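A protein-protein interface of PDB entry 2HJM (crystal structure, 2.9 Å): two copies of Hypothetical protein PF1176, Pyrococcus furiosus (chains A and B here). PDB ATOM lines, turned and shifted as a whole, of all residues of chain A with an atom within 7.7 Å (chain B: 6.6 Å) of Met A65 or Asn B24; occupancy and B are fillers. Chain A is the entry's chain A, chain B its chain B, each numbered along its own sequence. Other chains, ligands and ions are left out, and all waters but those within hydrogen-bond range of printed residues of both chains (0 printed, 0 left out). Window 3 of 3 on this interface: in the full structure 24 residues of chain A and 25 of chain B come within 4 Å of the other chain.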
ATOM      1  N   ILE A  59     -30.811 -35.563 -24.310  1.00  0.00           N
ATOM      2  CA  ILE A  59     -30.864 -35.241 -25.723  1.00  0.00           C
ATOM      3  C   ILE A  59     -31.107 -33.733 -25.906  1.00  0.00           C
ATOM      4  O   ILE A  59     -30.299 -33.028 -26.517  1.00  0.00           O
ATOM      5  CB  ILE A  59     -31.976 -36.036 -26.413  1.00  0.00           C
ATOM      6  CG1 ILE A  59     -31.506 -37.478 -26.621  1.00  0.00           C
ATOM      7  CG2 ILE A  59     -32.352 -35.384 -27.729  1.00  0.00           C
ATOM      8  CD1 ILE A  59     -32.585 -38.425 -27.121  1.00  0.00           C
ATOM      9  N   LEU A  60     -32.211 -33.239 -25.360  1.00  0.00           N
ATOM     10  CA  LEU A  60     -32.541 -31.831 -25.469  1.00  0.00           C
ATOM     11  C   LEU A  60     -31.439 -30.887 -25.008  1.00  0.00           C
ATOM     12  O   LEU A  60     -31.331 -29.766 -25.508  1.00  0.00           O
ATOM     13  CB  LEU A  60     -33.806 -31.535 -24.678  1.00  0.00           C
ATOM     14  CG  LEU A  60     -35.079 -32.171 -25.230  1.00  0.00           C
ATOM     15  CD1 LEU A  60     -36.251 -31.866 -24.306  1.00  0.00           C
ATOM     16  CD2 LEU A  60     -35.337 -31.634 -26.639  1.00  0.00           C
ATOM     17  N   THR A  61     -30.619 -31.326 -24.058  1.00  0.00           N
ATOM     18  CA  THR A  61     -29.554 -30.467 -23.553  1.00  0.00           C
ATOM     19  C   THR A  61     -28.360 -30.382 -24.479  1.00  0.00           C
ATOM     20  O   THR A  61     -27.829 -29.292 -24.692  1.00  0.00           O
ATOM     21  CB  THR A  61     -29.080 -30.901 -22.148  1.00  0.00           C
ATOM     22  OG1 THR A  61     -30.083 -30.557 -21.187  1.00  0.00           O
ATOM     23  CG2 THR A  61     -27.789 -30.193 -21.764  1.00  0.00           C
ATOM     24  N   THR A  62     -27.929 -31.499 -25.053  1.00  0.00           N
ATOM     25  CA  THR A  62     -26.771 -31.400 -25.934  1.00  0.00           C
ATOM     26  C   THR A  62     -27.116 -30.734 -27.274  1.00  0.00           C
ATOM     27  O   THR A  62     -26.233 -30.217 -27.955  1.00  0.00           O
ATOM     28  CB  THR A  62     -26.085 -32.781 -26.159  1.00  0.00           C
ATOM     29  OG1 THR A  62     -26.251 -33.204 -27.513  1.00  0.00           O
ATOM     30  CG2 THR A  62     -26.658 -33.810 -25.232  1.00  0.00           C
ATOM     31  N   LEU A  63     -28.395 -30.730 -27.647  1.00  0.00           N
ATOM     32  CA  LEU A  63     -28.814 -30.089 -28.896  1.00  0.00           C
ATOM     33  C   LEU A  63     -28.893 -28.592 -28.674  1.00  0.00           C
ATOM     34  O   LEU A  63     -28.557 -27.818 -29.563  1.00  0.00           O
ATOM     35  CB  LEU A  63     -30.187 -30.588 -29.370  1.00  0.00           C
ATOM     36  CG  LEU A  63     -30.251 -31.953 -30.054  1.00  0.00           C
ATOM     37  CD1 LEU A  63     -31.646 -32.206 -30.553  1.00  0.00           C
ATOM     38  CD2 LEU A  63     -29.295 -31.988 -31.209  1.00  0.00           C
ATOM     39  N   LYS A  64     -29.340 -28.188 -27.485  1.00  0.00           N
ATOM     40  CA  LYS A  64     -29.451 -26.773 -27.159  1.00  0.00           C
ATOM     41  C   LYS A  64     -28.066 -26.139 -27.174  1.00  0.00           C
ATOM     42  O   LYS A  64     -27.925 -24.940 -26.964  1.00  0.00           O
ATOM     43  CB  LYS A  64     -30.090 -26.599 -25.803  1.00  0.00           C
ATOM     44  N   MET A  65     -27.051 -26.963 -27.426  1.00  0.00           N
ATOM     45  CA  MET A  65     -25.657 -26.528 -27.491  1.00  0.00           C
ATOM     46  C   MET A  65     -25.193 -26.543 -28.948  1.00  0.00           C
ATOM     47  O   MET A  65     -24.051 -26.180 -29.252  1.00  0.00           O
ATOM     48  CB  MET A  65     -24.767 -27.476 -26.692  1.00  0.00           C
ATOM     49  CG  MET A  65     -25.198 -27.679 -25.263  1.00  0.00           C
ATOM     50  SD  MET A  65     -25.054 -26.069 -24.219  1.00  0.00           S
ATOM     51  CE  MET A  65     -26.903 -25.517 -24.212  1.00  0.00           C
ATOM     52  N   LYS A  66     -26.076 -26.996 -29.837  1.00  0.00           N
ATOM     53  CA  LYS A  66     -25.778 -27.060 -31.264  1.00  0.00           C
ATOM     54  C   LYS A  66     -26.675 -26.103 -32.060  1.00  0.00           C
ATOM     55  O   LYS A  66     -26.205 -25.398 -32.947  1.00  0.00           O
ATOM     56  CB  LYS A  66     -25.951 -28.492 -31.771  1.00  0.00           C
ATOM     57  N   TYR A  67     -27.962 -26.070 -31.730  1.00  0.00           N
ATOM     58  CA  TYR A  67     -28.903 -25.212 -32.429  1.00  0.00           C
ATOM     59  C   TYR A  67     -29.422 -24.105 -31.520  1.00  0.00           C
ATOM     60  O   TYR A  67     -29.037 -24.028 -30.356  1.00  0.00           O
ATOM     61  CB  TYR A  67     -30.056 -26.052 -32.968  1.00  0.00           C
ATOM     62  CG  TYR A  67     -29.599 -27.220 -33.810  1.00  0.00           C
ATOM     63  CD1 TYR A  67     -29.168 -28.406 -33.222  1.00  0.00           C
ATOM     64  CD2 TYR A  67     -29.557 -27.124 -35.195  1.00  0.00           C
ATOM     65  CE1 TYR A  67     -28.697 -29.476 -33.999  1.00  0.00           C
ATOM     66  CE2 TYR A  67     -29.089 -28.184 -35.983  1.00  0.00           C
ATOM     67  CZ  TYR A  67     -28.658 -29.355 -35.380  1.00  0.00           C
ATOM     68  OH  TYR A  67     -28.172 -30.384 -36.163  1.00  0.00           O
ATOM     69  N   SER A  68     -30.295 -23.251 -32.053  1.00  0.00           N
ATOM     70  CA  SER A  68     -30.844 -22.125 -31.290  1.00  0.00           C
ATOM     71  C   SER A  68     -32.370 -22.119 -31.204  1.00  0.00           C
ATOM     72  O   SER A  68     -32.949 -21.389 -30.392  1.00  0.00           O
ATOM     73  CB  SER A  68     -30.356 -20.807 -31.898  1.00  0.00           C
ATOM     74  N   ILE A  72     -36.485 -25.888 -28.667  1.00  0.00           N
ATOM     75  CA  ILE A  72     -35.636 -26.721 -27.821  1.00  0.00           C
ATOM     76  C   ILE A  72     -35.801 -26.401 -26.332  1.00  0.00           C
ATOM     77  O   ILE A  72     -36.123 -27.280 -25.534  1.00  0.00           O
ATOM     78  CB  ILE A  72     -34.130 -26.588 -28.196  1.00  0.00           C
ATOM     79  CG1 ILE A  72     -33.903 -27.028 -29.645  1.00  0.00           C
ATOM     80  CG2 ILE A  72     -33.288 -27.480 -27.304  1.00  0.00           C
ATOM     81  CD1 ILE A  72     -32.473 -26.879 -30.129  1.00  0.00           C
ATOM     82  N   LEU A  76     -37.348 -28.522 -23.587  1.00  0.00           N
ATOM     83  CA  LEU A  76     -36.497 -28.941 -22.491  1.00  0.00           C
ATOM     84  C   LEU A  76     -37.172 -28.652 -21.164  1.00  0.00           C
ATOM     85  O   LEU A  76     -37.167 -29.486 -20.266  1.00  0.00           O
ATOM     86  CB  LEU A  76     -35.159 -28.215 -22.560  1.00  0.00           C
ATOM     87  CG  LEU A  76     -34.192 -28.510 -21.412  1.00  0.00           C
ATOM     88  CD1 LEU A  76     -34.201 -29.994 -21.054  1.00  0.00           C
ATOM     89  CD2 LEU A  76     -32.802 -28.056 -21.826  1.00  0.00           C
ATOM     90  N   LEU B  18     -15.553 -31.882 -22.024  1.00  0.00           N
ATOM     91  CA  LEU B  18     -14.515 -30.865 -21.982  1.00  0.00           C
ATOM     92  C   LEU B  18     -13.538 -31.105 -23.114  1.00  0.00           C
ATOM     93  O   LEU B  18     -13.201 -30.180 -23.841  1.00  0.00           O
ATOM     94  CB  LEU B  18     -13.789 -30.899 -20.641  1.00  0.00           C
ATOM     95  CG  LEU B  18     -14.637 -30.539 -19.422  1.00  0.00           C
ATOM     96  CD1 LEU B  18     -13.787 -30.627 -18.193  1.00  0.00           C
ATOM     97  CD2 LEU B  18     -15.215 -29.147 -19.562  1.00  0.00           C
ATOM     98  N   GLU B  21     -14.616 -29.500 -26.235  1.00  0.00           N
ATOM     99  CA  GLU B  21     -14.898 -28.070 -26.206  1.00  0.00           C
ATOM    100  C   GLU B  21     -16.356 -27.724 -25.888  1.00  0.00           C
ATOM    101  O   GLU B  21     -16.819 -26.612 -26.167  1.00  0.00           O
ATOM    102  CB  GLU B  21     -14.481 -27.428 -27.529  1.00  0.00           C
ATOM    103  N   GLU B  22     -17.088 -28.664 -25.302  1.00  0.00           N
ATOM    104  CA  GLU B  22     -18.467 -28.382 -24.944  1.00  0.00           C
ATOM    105  C   GLU B  22     -18.607 -28.375 -23.436  1.00  0.00           C
ATOM    106  O   GLU B  22     -19.258 -29.239 -22.848  1.00  0.00           O
ATOM    107  CB  GLU B  22     -19.402 -29.401 -25.581  1.00  0.00           C
ATOM    108  CG  GLU B  22     -20.349 -28.746 -26.556  1.00  0.00           C
ATOM    109  CD  GLU B  22     -20.755 -29.674 -27.664  1.00  0.00           C
ATOM    110  OE1 GLU B  22     -19.855 -30.328 -28.225  1.00  0.00           O
ATOM    111  OE2 GLU B  22     -21.966 -29.748 -27.983  1.00  0.00           O
ATOM    112  N   GLU B  23     -17.986 -27.375 -22.824  1.00  0.00           N
ATOM    113  CA  GLU B  23     -17.989 -27.231 -21.378  1.00  0.00           C
ATOM    114  C   GLU B  23     -19.340 -26.882 -20.807  1.00  0.00           C
ATOM    115  O   GLU B  23     -19.616 -27.188 -19.647  1.00  0.00           O
ATOM    116  CB  GLU B  23     -16.977 -26.178 -20.953  1.00  0.00           C
ATOM    117  CG  GLU B  23     -17.197 -24.838 -21.594  1.00  0.00           C
ATOM    118  CD  GLU B  23     -16.192 -23.831 -21.117  1.00  0.00           C
ATOM    119  OE1 GLU B  23     -14.998 -24.189 -21.102  1.00  0.00           O
ATOM    120  OE2 GLU B  23     -16.583 -22.695 -20.761  1.00  0.00           O
ATOM    121  N   ASN B  24     -20.173 -26.217 -21.603  1.00  0.00           N
ATOM    122  CA  ASN B  24     -21.511 -25.869 -21.145  1.00  0.00           C
ATOM    123  C   ASN B  24     -22.225 -27.189 -20.915  1.00  0.00           C
ATOM    124  O   ASN B  24     -22.914 -27.386 -19.911  1.00  0.00           O
ATOM    125  CB  ASN B  24     -22.269 -25.063 -22.204  1.00  0.00           C
ATOM    126  CG  ASN B  24     -22.051 -23.570 -22.068  1.00  0.00           C
ATOM    127  OD1 ASN B  24     -21.917 -23.046 -20.954  1.00  0.00           O
ATOM    128  ND2 ASN B  24     -22.040 -22.869 -23.198  1.00  0.00           N
ATOM    129  N   LEU B  25     -22.046 -28.092 -21.871  1.00  0.00           N
ATOM    130  CA  LEU B  25     -22.642 -29.405 -21.788  1.00  0.00           C
ATOM    131  C   LEU B  25     -22.172 -29.973 -20.458  1.00  0.00           C
ATOM    132  O   LEU B  25     -22.962 -30.490 -19.676  1.00  0.00           O
ATOM    133  CB  LEU B  25     -22.149 -30.263 -22.951  1.00  0.00           C
ATOM    134  CG  LEU B  25     -23.034 -31.428 -23.401  1.00  0.00           C
ATOM    135  CD1 LEU B  25     -24.507 -31.020 -23.368  1.00  0.00           C
ATOM    136  CD2 LEU B  25     -22.613 -31.859 -24.808  1.00  0.00           C
ATOM    137  N   ALA B  26     -20.879 -29.840 -20.192  1.00  0.00           N
ATOM    138  CA  ALA B  26     -20.301 -30.328 -18.951  1.00  0.00           C
ATOM    139  C   ALA B  26     -20.904 -29.637 -17.732  1.00  0.00           C
ATOM    140  O   ALA B  26     -21.174 -30.273 -16.714  1.00  0.00           O
ATOM    141  CB  ALA B  26     -18.809 -30.126 -18.968  1.00  0.00           C
ATOM    142  N   LYS B  27     -21.120 -28.333 -17.817  1.00  0.00           N
ATOM    143  CA  LYS B  27     -21.682 -27.634 -16.670  1.00  0.00           C
ATOM    144  C   LYS B  27     -23.103 -28.146 -16.404  1.00  0.00           C
ATOM    145  O   LYS B  27     -23.567 -28.185 -15.261  1.00  0.00           O
ATOM    146  CB  LYS B  27     -21.667 -26.117 -16.915  1.00  0.00           C
ATOM    147  N   ALA B  28     -23.784 -28.553 -17.474  1.00  0.00           N
ATOM    148  CA  ALA B  28     -25.144 -29.072 -17.363  1.00  0.00           C
ATOM    149  C   ALA B  28     -25.132 -30.334 -16.507  1.00  0.00           C
ATOM    150  O   ALA B  28     -25.854 -30.430 -15.514  1.00  0.00           O
ATOM    151  CB  ALA B  28     -25.700 -29.373 -18.736  1.00  0.00           C
ATOM    152  N   ILE B  29     -24.312 -31.304 -16.894  1.00  0.00           N
ATOM    153  CA  ILE B  29     -24.212 -32.540 -16.139  1.00  0.00           C
ATOM    154  C   ILE B  29     -24.038 -32.177 -14.676  1.00  0.00           C
ATOM    155  O   ILE B  29     -24.642 -32.771 -13.793  1.00  0.00           O
ATOM    156  CB  ILE B  29     -23.001 -33.372 -16.605  1.00  0.00           C
ATOM    157  CG1 ILE B  29     -23.209 -33.799 -18.057  1.00  0.00           C
ATOM    158  CG2 ILE B  29     -22.798 -34.580 -15.700  1.00  0.00           C
ATOM    159  CD1 ILE B  29     -22.057 -34.598 -18.637  1.00  0.00           C
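No position is printed for both chains.
Of the 6 pairs that touch across the chains among the printed residues, none has its exchanged pair printed and touching as well.
Met A65 touches three residues of chain B.
Of the printed residues of chain A, Asn B24 touches Met A65.
Printed residues of chain B within 4 Å of Thr A61: Leu B25 (3.7 Å) and Ala B28 (3.8 Å).
Of the printed residues of chain A, Ala B28 touches Thr A61.
Of the printed residues of chain B, Thr A62 touches Leu B25.
Of the printed residues of chain A, Leu B25 touches Thr A61, Thr A62 and Met A65.
The nearest residue of chain B that does not touch Met A65 is Ala B28 (6.4 Å).
The nearest residue of chain A that does not touch Asn B24 is Thr A61 (5.9 Å).
Of the 12 printed residues of chain A, 3 touch a printed residue of chain B.
Hydrophobic or aromatic side chains of chain A that line the printed part of chain B: Met A65.
Among the printed residues, no Asp or Glu carboxylate lies within 4 Å of a Lys or Arg side-chain nitrogen of the other chain.
Leu B25 touches Thr A61 (CD1 to CG2, 3.7 Å).
CB of Ala B28 touches CG2 of Thr A61 (3.8 Å).
Thr A62 touches Leu B25 (CA to CD1, 3.4 Å).
Met A65 touches Glu B22 (CB to OE2, 3.8 Å).
Asn B24 touches Met A65 (CB to SD, 3.6 Å).
Met A65 touches Leu B25.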
